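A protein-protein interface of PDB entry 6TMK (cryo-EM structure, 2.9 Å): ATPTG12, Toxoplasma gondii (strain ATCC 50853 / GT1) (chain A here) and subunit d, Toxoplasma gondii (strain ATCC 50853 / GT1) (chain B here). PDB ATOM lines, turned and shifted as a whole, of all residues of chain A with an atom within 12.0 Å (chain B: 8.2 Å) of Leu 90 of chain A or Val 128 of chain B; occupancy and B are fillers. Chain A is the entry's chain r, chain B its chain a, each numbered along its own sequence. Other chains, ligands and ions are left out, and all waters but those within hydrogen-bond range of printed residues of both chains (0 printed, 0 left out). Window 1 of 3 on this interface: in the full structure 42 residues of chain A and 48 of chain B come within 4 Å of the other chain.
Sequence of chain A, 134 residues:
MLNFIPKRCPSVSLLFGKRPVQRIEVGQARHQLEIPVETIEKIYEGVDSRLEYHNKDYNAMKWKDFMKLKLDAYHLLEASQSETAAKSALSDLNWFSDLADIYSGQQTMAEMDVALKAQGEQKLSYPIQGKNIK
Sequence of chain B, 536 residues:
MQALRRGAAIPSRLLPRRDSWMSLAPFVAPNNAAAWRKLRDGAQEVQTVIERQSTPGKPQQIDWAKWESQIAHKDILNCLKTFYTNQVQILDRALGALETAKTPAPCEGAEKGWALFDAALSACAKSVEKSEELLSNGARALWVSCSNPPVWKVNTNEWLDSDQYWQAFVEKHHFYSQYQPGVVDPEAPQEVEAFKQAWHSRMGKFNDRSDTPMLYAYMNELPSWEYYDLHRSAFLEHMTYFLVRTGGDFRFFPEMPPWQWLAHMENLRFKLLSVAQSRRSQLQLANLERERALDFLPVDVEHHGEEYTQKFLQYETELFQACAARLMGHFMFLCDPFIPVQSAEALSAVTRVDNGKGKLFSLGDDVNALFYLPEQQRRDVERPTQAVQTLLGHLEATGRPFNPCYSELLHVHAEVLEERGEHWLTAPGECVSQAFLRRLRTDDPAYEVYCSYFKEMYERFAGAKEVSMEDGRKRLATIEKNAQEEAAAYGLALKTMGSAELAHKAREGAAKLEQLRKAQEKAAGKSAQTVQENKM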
ATOM      1  N   THR A  39       7.079  -5.310   5.629  1.00  0.00           N
ATOM      2  CA  THR A  39       6.502  -5.546   6.943  1.00  0.00           C
ATOM      3  C   THR A  39       5.703  -4.339   7.403  1.00  0.00           C
ATOM      4  O   THR A  39       4.640  -4.484   8.016  1.00  0.00           O
ATOM      5  CB  THR A  39       7.610  -5.860   7.946  1.00  0.00           C
ATOM      6  OG1 THR A  39       8.178  -7.141   7.654  1.00  0.00           O
ATOM      7  CG2 THR A  39       7.073  -5.857   9.356  1.00  0.00           C
ATOM      8  N   ASP A  72      -0.097  -9.205  20.470  1.00  0.00           N
ATOM      9  CA  ASP A  72       1.250  -9.717  20.247  1.00  0.00           C
ATOM     10  C   ASP A  72       2.260  -8.989  21.126  1.00  0.00           C
ATOM     11  O   ASP A  72       3.117  -9.620  21.767  1.00  0.00           O
ATOM     12  CB  ASP A  72       1.618  -9.583  18.775  1.00  0.00           C
ATOM     13  CG  ASP A  72       0.767 -10.465  17.883  1.00  0.00           C
ATOM     14  OD1 ASP A  72      -0.349 -10.836  18.304  1.00  0.00           O
ATOM     15  OD2 ASP A  72       1.212 -10.790  16.763  1.00  0.00           O
ATOM     16  N   LEU A  76       4.456 -10.773  24.206  1.00  0.00           N
ATOM     17  CA  LEU A  76       5.907 -10.669  24.321  1.00  0.00           C
ATOM     18  C   LEU A  76       6.311 -10.041  25.648  1.00  0.00           C
ATOM     19  O   LEU A  76       7.269 -10.488  26.291  1.00  0.00           O
ATOM     20  CB  LEU A  76       6.471  -9.865  23.155  1.00  0.00           C
ATOM     21  CG  LEU A  76       6.352 -10.516  21.782  1.00  0.00           C
ATOM     22  CD1 LEU A  76       6.728  -9.541  20.709  1.00  0.00           C
ATOM     23  CD2 LEU A  76       7.231 -11.738  21.701  1.00  0.00           C
ATOM     24  N   ALA A  79       5.743 -12.483  28.546  1.00  0.00           N
ATOM     25  CA  ALA A  79       6.774 -13.509  28.456  1.00  0.00           C
ATOM     26  C   ALA A  79       8.105 -12.992  28.982  1.00  0.00           C
ATOM     27  O   ALA A  79       8.831 -13.712  29.676  1.00  0.00           O
ATOM     28  CB  ALA A  79       6.918 -13.979  27.013  1.00  0.00           C
ATOM     29  N   THR A  84       9.075 -18.797  33.401  1.00  0.00           N
ATOM     30  CA  THR A  84       8.774 -20.048  32.719  1.00  0.00           C
ATOM     31  C   THR A  84       8.433 -19.847  31.250  1.00  0.00           C
ATOM     32  O   THR A  84       7.826 -20.733  30.637  1.00  0.00           O
ATOM     33  CB  THR A  84       7.623 -20.767  33.426  1.00  0.00           C
ATOM     34  OG1 THR A  84       7.546 -22.121  32.963  1.00  0.00           O
ATOM     35  CG2 THR A  84       6.301 -20.065  33.149  1.00  0.00           C
ATOM     36  N   ALA A  85       8.808 -18.707  30.677  1.00  0.00           N
ATOM     37  CA  ALA A  85       8.511 -18.441  29.280  1.00  0.00           C
ATOM     38  C   ALA A  85       9.238 -19.429  28.379  1.00  0.00           C
ATOM     39  O   ALA A  85      10.345 -19.884  28.676  1.00  0.00           O
ATOM     40  CB  ALA A  85       8.916 -17.015  28.919  1.00  0.00           C
ATOM     41  N   ALA A  86       8.598 -19.759  27.261  1.00  0.00           N
ATOM     42  CA  ALA A  86       9.209 -20.653  26.291  1.00  0.00           C
ATOM     43  C   ALA A  86      10.480 -20.036  25.729  1.00  0.00           C
ATOM     44  O   ALA A  86      10.553 -18.829  25.483  1.00  0.00           O
ATOM     45  CB  ALA A  86       8.227 -20.958  25.161  1.00  0.00           C
ATOM     46  N   LYS A  87      11.494 -20.878  25.529  1.00  0.00           N
ATOM     47  CA  LYS A  87      12.743 -20.427  24.931  1.00  0.00           C
ATOM     48  C   LYS A  87      12.613 -20.158  23.441  1.00  0.00           C
ATOM     49  O   LYS A  87      13.567 -19.658  22.836  1.00  0.00           O
ATOM     50  CB  LYS A  87      13.836 -21.467  25.170  1.00  0.00           C
ATOM     51  CG  LYS A  87      14.215 -21.632  26.629  1.00  0.00           C
ATOM     52  CD  LYS A  87      15.099 -20.497  27.108  1.00  0.00           C
ATOM     53  CE  LYS A  87      14.894 -20.224  28.589  1.00  0.00           C
ATOM     54  NZ  LYS A  87      13.587 -19.567  28.866  1.00  0.00           N
ATOM     55  N   SER A  88      11.471 -20.474  22.838  1.00  0.00           N
ATOM     56  CA  SER A  88      11.262 -20.226  21.422  1.00  0.00           C
ATOM     57  C   SER A  88       9.788 -19.970  21.154  1.00  0.00           C
ATOM     58  O   SER A  88       8.913 -20.444  21.885  1.00  0.00           O
ATOM     59  CB  SER A  88      11.743 -21.407  20.577  1.00  0.00           C
ATOM     60  OG  SER A  88      11.436 -21.205  19.211  1.00  0.00           O
ATOM     61  N   ALA A  89       9.526 -19.214  20.091  1.00  0.00           N
ATOM     62  CA  ALA A  89       8.168 -18.896  19.680  1.00  0.00           C
ATOM     63  C   ALA A  89       7.539 -20.001  18.848  1.00  0.00           C
ATOM     64  O   ALA A  89       6.336 -19.942  18.570  1.00  0.00           O
ATOM     65  CB  ALA A  89       8.152 -17.593  18.884  1.00  0.00           C
ATOM     66  N   LEU A  90       8.322 -20.995  18.448  1.00  0.00           N
ATOM     67  CA  LEU A  90       7.824 -22.080  17.624  1.00  0.00           C
ATOM     68  C   LEU A  90       6.893 -22.983  18.425  1.00  0.00           C
ATOM     69  O   LEU A  90       6.953 -23.057  19.655  1.00  0.00           O
ATOM     70  CB  LEU A  90       8.990 -22.896  17.076  1.00  0.00           C
ATOM     71  CG  LEU A  90       9.928 -22.151  16.129  1.00  0.00           C
ATOM     72  CD1 LEU A  90      11.212 -22.925  15.941  1.00  0.00           C
ATOM     73  CD2 LEU A  90       9.260 -21.905  14.793  1.00  0.00           C
ATOM     74  N   SER A  91       6.025 -23.682  17.702  1.00  0.00           N
ATOM     75  CA  SER A  91       5.111 -24.621  18.323  1.00  0.00           C
ATOM     76  C   SER A  91       5.846 -25.913  18.656  1.00  0.00           C
ATOM     77  O   SER A  91       7.013 -26.104  18.306  1.00  0.00           O
ATOM     78  CB  SER A  91       3.923 -24.905  17.406  1.00  0.00           C
ATOM     79  OG  SER A  91       3.187 -23.728  17.143  1.00  0.00           O
ATOM     80  N   ASP A  92       5.160 -26.799  19.370  1.00  0.00           N
ATOM     81  CA  ASP A  92       5.766 -28.059  19.764  1.00  0.00           C
ATOM     82  C   ASP A  92       6.309 -28.796  18.548  1.00  0.00           C
ATOM     83  O   ASP A  92       5.624 -28.947  17.534  1.00  0.00           O
ATOM     84  CB  ASP A  92       4.739 -28.925  20.492  1.00  0.00           C
ATOM     85  CG  ASP A  92       5.227 -30.344  20.718  1.00  0.00           C
ATOM     86  OD1 ASP A  92       5.028 -31.193  19.823  1.00  0.00           O
ATOM     87  OD2 ASP A  92       5.805 -30.611  21.792  1.00  0.00           O
ATOM     88  N   LEU A  93       7.554 -29.248  18.661  1.00  0.00           N
ATOM     89  CA  LEU A  93       8.236 -29.957  17.589  1.00  0.00           C
ATOM     90  C   LEU A  93       8.048 -31.452  17.794  1.00  0.00           C
ATOM     91  O   LEU A  93       8.199 -31.953  18.912  1.00  0.00           O
ATOM     92  CB  LEU A  93       9.723 -29.604  17.558  1.00  0.00           C
ATOM     93  CG  LEU A  93      10.102 -28.455  16.626  1.00  0.00           C
ATOM     94  CD1 LEU A  93       9.450 -27.173  17.071  1.00  0.00           C
ATOM     95  CD2 LEU A  93      11.605 -28.284  16.581  1.00  0.00           C
ATOM     96  N   ASN A  94       7.689 -32.157  16.719  1.00  0.00           N
ATOM     97  CA  ASN A  94       7.386 -33.578  16.828  1.00  0.00           C
ATOM     98  C   ASN A  94       7.978 -34.387  15.680  1.00  0.00           C
ATOM     99  O   ASN A  94       7.508 -35.501  15.416  1.00  0.00           O
ATOM    100  CB  ASN A  94       5.873 -33.791  16.882  1.00  0.00           C
ATOM    101  CG  ASN A  94       5.154 -33.122  15.731  1.00  0.00           C
ATOM    102  OD1 ASN A  94       5.782 -32.538  14.849  1.00  0.00           O
ATOM    103  ND2 ASN A  94       3.829 -33.200  15.735  1.00  0.00           N
ATOM    104  N   TRP A  95       8.994 -33.865  14.994  1.00  0.00           N
ATOM    105  CA  TRP A  95       9.592 -34.542  13.851  1.00  0.00           C
ATOM    106  C   TRP A  95      11.059 -34.891  14.093  1.00  0.00           C
ATOM    107  O   TRP A  95      11.853 -34.951  13.154  1.00  0.00           O
ATOM    108  CB  TRP A  95       9.429 -33.705  12.583  1.00  0.00           C
ATOM    109  CG  TRP A  95       9.578 -32.229  12.777  1.00  0.00           C
ATOM    110  CD1 TRP A  95       8.593 -31.292  12.676  1.00  0.00           C
ATOM    111  CD2 TRP A  95      10.783 -31.513  13.068  1.00  0.00           C
ATOM    112  NE1 TRP A  95       9.104 -30.041  12.904  1.00  0.00           N
ATOM    113  CE2 TRP A  95      10.447 -30.148  13.144  1.00  0.00           C
ATOM    114  CE3 TRP A  95      12.110 -31.893  13.276  1.00  0.00           C
ATOM    115  CZ2 TRP A  95      11.390 -29.164  13.422  1.00  0.00           C
ATOM    116  CZ3 TRP A  95      13.043 -30.914  13.555  1.00  0.00           C
ATOM    117  CH2 TRP A  95      12.679 -29.566  13.624  1.00  0.00           C
ATOM    118  N   PHE A  96      11.429 -35.135  15.350  1.00  0.00           N
ATOM    119  CA  PHE A  96      12.748 -35.669  15.665  1.00  0.00           C
ATOM    120  C   PHE A  96      12.760 -37.189  15.682  1.00  0.00           C
ATOM    121  O   PHE A  96      13.795 -37.803  15.378  1.00  0.00           O
ATOM    122  CB  PHE A  96      13.216 -35.151  17.028  1.00  0.00           C
ATOM    123  CG  PHE A  96      13.539 -33.689  17.046  1.00  0.00           C
ATOM    124  CD1 PHE A  96      14.552 -33.180  16.255  1.00  0.00           C
ATOM    125  CD2 PHE A  96      12.828 -32.820  17.855  1.00  0.00           C
ATOM    126  CE1 PHE A  96      14.851 -31.836  16.271  1.00  0.00           C
ATOM    127  CE2 PHE A  96      13.125 -31.474  17.874  1.00  0.00           C
ATOM    128  CZ  PHE A  96      14.138 -30.982  17.081  1.00  0.00           C
ATOM    129  N   LEU B  24      21.431 -27.974  15.870  1.00  0.00           N
ATOM    130  CA  LEU B  24      19.986 -27.926  16.032  1.00  0.00           C
ATOM    131  C   LEU B  24      19.548 -28.330  17.436  1.00  0.00           C
ATOM    132  O   LEU B  24      18.382 -28.684  17.640  1.00  0.00           O
ATOM    133  CB  LEU B  24      19.332 -28.828  14.984  1.00  0.00           C
ATOM    134  CG  LEU B  24      17.813 -28.935  14.899  1.00  0.00           C
ATOM    135  CD1 LEU B  24      17.178 -27.572  15.003  1.00  0.00           C
ATOM    136  CD2 LEU B  24      17.420 -29.609  13.602  1.00  0.00           C
ATOM    137  N   PHE B  27      16.672 -26.105  19.907  1.00  0.00           N
ATOM    138  CA  PHE B  27      15.289 -26.251  19.478  1.00  0.00           C
ATOM    139  C   PHE B  27      14.686 -27.588  19.882  1.00  0.00           C
ATOM    140  O   PHE B  27      13.560 -27.893  19.475  1.00  0.00           O
ATOM    141  CB  PHE B  27      15.199 -26.070  17.963  1.00  0.00           C
ATOM    142  CG  PHE B  27      15.814 -24.796  17.473  1.00  0.00           C
ATOM    143  CD1 PHE B  27      15.089 -23.621  17.478  1.00  0.00           C
ATOM    144  CD2 PHE B  27      17.120 -24.766  17.027  1.00  0.00           C
ATOM    145  CE1 PHE B  27      15.651 -22.445  17.033  1.00  0.00           C
ATOM    146  CE2 PHE B  27      17.687 -23.595  16.580  1.00  0.00           C
ATOM    147  CZ  PHE B  27      16.952 -22.431  16.585  1.00  0.00           C
ATOM    148  N   LEU B 121       9.822 -31.018   7.181  1.00  0.00           N
ATOM    149  CA  LEU B 121      10.263 -29.720   6.691  1.00  0.00           C
ATOM    150  C   LEU B 121       9.077 -28.786   6.510  1.00  0.00           C
ATOM    151  O   LEU B 121       9.158 -27.595   6.826  1.00  0.00           O
ATOM    152  CB  LEU B 121      11.014 -29.899   5.374  1.00  0.00           C
ATOM    153  CG  LEU B 121      11.671 -28.666   4.764  1.00  0.00           C
ATOM    154  CD1 LEU B 121      12.974 -28.358   5.469  1.00  0.00           C
ATOM    155  CD2 LEU B 121      11.903 -28.878   3.281  1.00  0.00           C
ATOM    156  N   SER B 122       7.968 -29.311   5.990  1.00  0.00           N
ATOM    157  CA  SER B 122       6.780 -28.488   5.788  1.00  0.00           C
ATOM    158  C   SER B 122       6.247 -27.970   7.117  1.00  0.00           C
ATOM    159  O   SER B 122       5.925 -26.780   7.253  1.00  0.00           O
ATOM    160  CB  SER B 122       5.708 -29.291   5.055  1.00  0.00           C
ATOM    161  OG  SER B 122       5.762 -29.058   3.660  1.00  0.00           O
ATOM    162  N   ALA B 123       6.186 -28.844   8.123  1.00  0.00           N
ATOM    163  CA  ALA B 123       5.710 -28.422   9.437  1.00  0.00           C
ATOM    164  C   ALA B 123       6.656 -27.407  10.062  1.00  0.00           C
ATOM    165  O   ALA B 123       6.213 -26.434  10.688  1.00  0.00           O
ATOM    166  CB  ALA B 123       5.546 -29.633  10.350  1.00  0.00           C
ATOM    167  N   CYS B 124       7.963 -27.610   9.897  1.00  0.00           N
ATOM    168  CA  CYS B 124       8.920 -26.676  10.474  1.00  0.00           C
ATOM    169  C   CYS B 124       8.806 -25.318   9.803  1.00  0.00           C
ATOM    170  O   CYS B 124       8.886 -24.281  10.469  1.00  0.00           O
ATOM    171  CB  CYS B 124      10.339 -27.221  10.335  1.00  0.00           C
ATOM    172  SG  CYS B 124      11.623 -26.050  10.816  1.00  0.00           S
ATOM    173  N   ALA B 125       8.634 -25.305   8.480  1.00  0.00           N
ATOM    174  CA  ALA B 125       8.470 -24.044   7.774  1.00  0.00           C
ATOM    175  C   ALA B 125       7.197 -23.336   8.212  1.00  0.00           C
ATOM    176  O   ALA B 125       7.176 -22.109   8.333  1.00  0.00           O
ATOM    177  CB  ALA B 125       8.453 -24.287   6.269  1.00  0.00           C
ATOM    178  N   LYS B 126       6.130 -24.093   8.477  1.00  0.00           N
ATOM    179  CA  LYS B 126       4.896 -23.466   8.945  1.00  0.00           C
ATOM    180  C   LYS B 126       5.070 -22.858  10.335  1.00  0.00           C
ATOM    181  O   LYS B 126       4.585 -21.748  10.608  1.00  0.00           O
ATOM    182  CB  LYS B 126       3.764 -24.487   8.950  1.00  0.00           C
ATOM    183  CG  LYS B 126       2.416 -23.895   9.296  1.00  0.00           C
ATOM    184  CD  LYS B 126       1.291 -24.878   9.040  1.00  0.00           C
ATOM    185  CE  LYS B 126       1.322 -26.020  10.037  1.00  0.00           C
ATOM    186  NZ  LYS B 126       0.161 -26.934   9.868  1.00  0.00           N
ATOM    187  N   SER B 127       5.766 -23.569  11.224  1.00  0.00           N
ATOM    188  CA  SER B 127       6.044 -23.029  12.550  1.00  0.00           C
ATOM    189  C   SER B 127       6.901 -21.773  12.461  1.00  0.00           C
ATOM    190  O   SER B 127       6.631 -20.769  13.132  1.00  0.00           O
ATOM    191  CB  SER B 127       6.734 -24.088  13.406  1.00  0.00           C
ATOM    192  OG  SER B 127       5.894 -25.212  13.595  1.00  0.00           O
ATOM    193  N   VAL B 128       7.951 -21.817  11.641  1.00  0.00           N
ATOM    194  CA  VAL B 128       8.789 -20.642  11.448  1.00  0.00           C
ATOM    195  C   VAL B 128       7.969 -19.505  10.868  1.00  0.00           C
ATOM    196  O   VAL B 128       8.183 -18.338  11.207  1.00  0.00           O
ATOM    197  CB  VAL B 128       9.989 -20.986  10.548  1.00  0.00           C
ATOM    198  CG1 VAL B 128      10.695 -19.724  10.103  1.00  0.00           C
ATOM    199  CG2 VAL B 128      10.948 -21.897  11.280  1.00  0.00           C
ATOM    200  N   GLU B 129       7.002 -19.825  10.012  1.00  0.00           N
ATOM    201  CA  GLU B 129       6.172 -18.797   9.401  1.00  0.00           C
ATOM    202  C   GLU B 129       5.341 -18.080  10.451  1.00  0.00           C
ATOM    203  O   GLU B 129       5.299 -16.845  10.489  1.00  0.00           O
ATOM    204  CB  GLU B 129       5.272 -19.427   8.339  1.00  0.00           C
ATOM    205  CG  GLU B 129       4.393 -18.438   7.605  1.00  0.00           C
ATOM    206  CD  GLU B 129       2.991 -18.372   8.177  1.00  0.00           C
ATOM    207  OE1 GLU B 129       2.375 -19.442   8.369  1.00  0.00           O
ATOM    208  OE2 GLU B 129       2.504 -17.252   8.436  1.00  0.00           O
ATOM    209  N   LYS B 130       4.663 -18.837  11.312  1.00  0.00           N
ATOM    210  CA  LYS B 130       3.821 -18.174  12.303  1.00  0.00           C
ATOM    211  C   LYS B 130       4.658 -17.461  13.362  1.00  0.00           C
ATOM    212  O   LYS B 130       4.251 -16.406  13.867  1.00  0.00           O
ATOM    213  CB  LYS B 130       2.852 -19.171  12.936  1.00  0.00           C
ATOM    214  CG  LYS B 130       3.476 -20.278  13.734  1.00  0.00           C
ATOM    215  CD  LYS B 130       3.559 -19.908  15.199  1.00  0.00           C
ATOM    216  CE  LYS B 130       4.087 -21.055  16.026  1.00  0.00           C
ATOM    217  NZ  LYS B 130       4.266 -20.685  17.456  1.00  0.00           N
ATOM    218  N   SER B 131       5.840 -17.987  13.696  1.00  0.00           N
ATOM    219  CA  SER B 131       6.705 -17.270  14.629  1.00  0.00           C
ATOM    220  C   SER B 131       7.216 -15.973  14.011  1.00  0.00           C
ATOM    221  O   SER B 131       7.334 -14.948  14.699  1.00  0.00           O
ATOM    222  CB  SER B 131       7.873 -18.151  15.055  1.00  0.00           C
ATOM    223  OG  SER B 131       8.723 -18.422  13.960  1.00  0.00           O
ATOM    224  N   GLU B 132       7.524 -15.997  12.714  1.00  0.00           N
ATOM    225  CA  GLU B 132       7.901 -14.774  12.024  1.00  0.00           C
ATOM    226  C   GLU B 132       6.741 -13.800  11.977  1.00  0.00           C
ATOM    227  O   GLU B 132       6.952 -12.590  12.043  1.00  0.00           O
ATOM    228  CB  GLU B 132       8.384 -15.089  10.612  1.00  0.00           C
ATOM    229  CG  GLU B 132       9.815 -15.574  10.552  1.00  0.00           C
ATOM    230  CD  GLU B 132      10.265 -15.884   9.139  1.00  0.00           C
ATOM    231  OE1 GLU B 132       9.436 -15.769   8.211  1.00  0.00           O
ATOM    232  OE2 GLU B 132      11.448 -16.240   8.955  1.00  0.00           O
ATOM    233  N   GLU B 133       5.514 -14.305  11.852  1.00  0.00           N
ATOM    234  CA  GLU B 133       4.351 -13.429  11.923  1.00  0.00           C
ATOM    235  C   GLU B 133       4.281 -12.747  13.279  1.00  0.00           C
ATOM    236  O   GLU B 133       4.024 -11.541  13.369  1.00  0.00           O
ATOM    237  CB  GLU B 133       3.077 -14.228  11.658  1.00  0.00           C
ATOM    238  CG  GLU B 133       1.820 -13.381  11.519  1.00  0.00           C
ATOM    239  CD  GLU B 133       1.825 -12.514  10.278  1.00  0.00           C
ATOM    240  OE1 GLU B 133       2.593 -12.818   9.340  1.00  0.00           O
ATOM    241  OE2 GLU B 133       1.059 -11.529  10.238  1.00  0.00           O
ATOM    242  N   LEU B 134       4.513 -13.507  14.349  1.00  0.00           N
ATOM    243  CA  LEU B 134       4.520 -12.922  15.685  1.00  0.00           C
ATOM    244  C   LEU B 134       5.570 -11.824  15.798  1.00  0.00           C
ATOM    245  O   LEU B 134       5.285 -10.715  16.270  1.00  0.00           O
ATOM    246  CB  LEU B 134       4.777 -14.007  16.725  1.00  0.00           C
ATOM    247  CG  LEU B 134       4.696 -13.558  18.182  1.00  0.00           C
ATOM    248  CD1 LEU B 134       3.262 -13.500  18.650  1.00  0.00           C
ATOM    249  CD2 LEU B 134       5.500 -14.483  19.055  1.00  0.00           C
ATOM    250  N   LEU B 135       6.805 -12.124  15.397  1.00  0.00           N
ATOM    251  CA  LEU B 135       7.869 -11.136  15.544  1.00  0.00           C
ATOM    252  C   LEU B 135       7.663  -9.944  14.622  1.00  0.00           C
ATOM    253  O   LEU B 135       8.034  -8.818  14.971  1.00  0.00           O
ATOM    254  CB  LEU B 135       9.225 -11.778  15.286  1.00  0.00           C
ATOM    255  CG  LEU B 135       9.871 -12.344  16.545  1.00  0.00           C
ATOM    256  CD1 LEU B 135       9.161 -13.607  16.963  1.00  0.00           C
ATOM    257  CD2 LEU B 135      11.340 -12.600  16.315  1.00  0.00           C
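The side-chain amino group (NZ) of Lys 130 of chain B sits close to the side-chain hydroxyl (OG) of Ser 91 of chain A (3.2 Å). NZ of Lys 130 of chain B lies within hydrogen-bond range of O of Ala 89 of chain A (2.5 Å).
OG of Ser 131 of chain B lies within hydrogen-bond range of O of Val 128 of chain B (2.8 Å). The backbone carbonyl oxygen of Ser 127 of chain B sits at hydrogen-bond distance from the side-chain hydroxyl of Ser 131 of chain B. OG of Ser 88 of chain A sits at hydrogen-bond distance from N of Leu 90 of chain A. The side-chain hydroxyl (OG) of Ser 127 of chain B is in hydrogen-bond range of the backbone carbonyl oxygen (O) of Ala 123 of chain B, 3.2 Å away.
Among the printed residues, pairs that only touch across the chains: Leu 90 of chain A with Ser 127 of chain B, Leu 90 of chain A with Val 128 of chain B, Leu 93 of chain A with Phe 27 of chain B, Leu 90 of chain A with Ser 131 of chain B, Leu 90 of chain A with Lys 130 of chain B, Trp 95 of chain A with Cys 124 of chain B, Ala 89 of chain A with Ser 131 of chain B, Asp 72 of chain A with Leu 134 of chain B and Phe 96 of chain A with Phe 27 of chain B.
Of the printed residues of chain B, Asp 72 of chain A touches Leu 134 (3.9 Å). Ala 86 of chain A touches none of the printed residues of chain B. Ser 88 of chain A touches none of the printed residues of chain B. Ala 89 of chain A touches just these residues of chain B: Lys 130 and Ser 131. Leu 90 of chain A touches just these residues of chain B: Ser 127, Val 128, Lys 130 and Ser 131. Of the printed residues of chain B, Leu 93 of chain A touches Phe 27. Of the printed residues of chain B, Trp 95 of chain A touches Cys 124. Of chain A, only Leu 93 and Phe 96 come within 4 Å of Phe 27 of chain B. No residue of chain A comes within 4 Å of Ala 125 of chain B. Of the printed residues of chain A, Val 128 of chain B touches Leu 90. No residue of chain A comes within 4 Å of Glu 129 of chain B. Ser 131 of chain B touches just these residues of chain A: Ala 89 (3.9 Å) and Leu 90 (3.6 Å). No residue of chain A comes within 4 Å of Glu 132 of chain B. Of the printed residues of chain A, Leu 134 of chain B touches Asp 72 (3.9 Å). The nearest printed residue of chain B that does not touch Phe 96 of chain A is Leu 24 of chain B (4.3 Å).
Of the 17 printed residues of chain B, 7 touch a printed residue of chain A. Printed residues of chain B that touch a printed residue of chain A: Phe 27, Cys 124, Ser 127, Val 128, Lys 130, Ser 131 and Leu 134. Of the 17 printed residues of chain A, 7 touch a printed residue of chain B. Hydrophobic or aromatic side chains of chain A within 4 Å of the printed part of chain B: Ala 89, Leu 90, Leu 93, Trp 95 and Phe 96. Among the printed residues, 11 pairs touch across the chains. Among the printed residues, no Asp or Glu carboxylate lies within 4 Å of a Lys or Arg side-chain nitrogen of the other chain.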
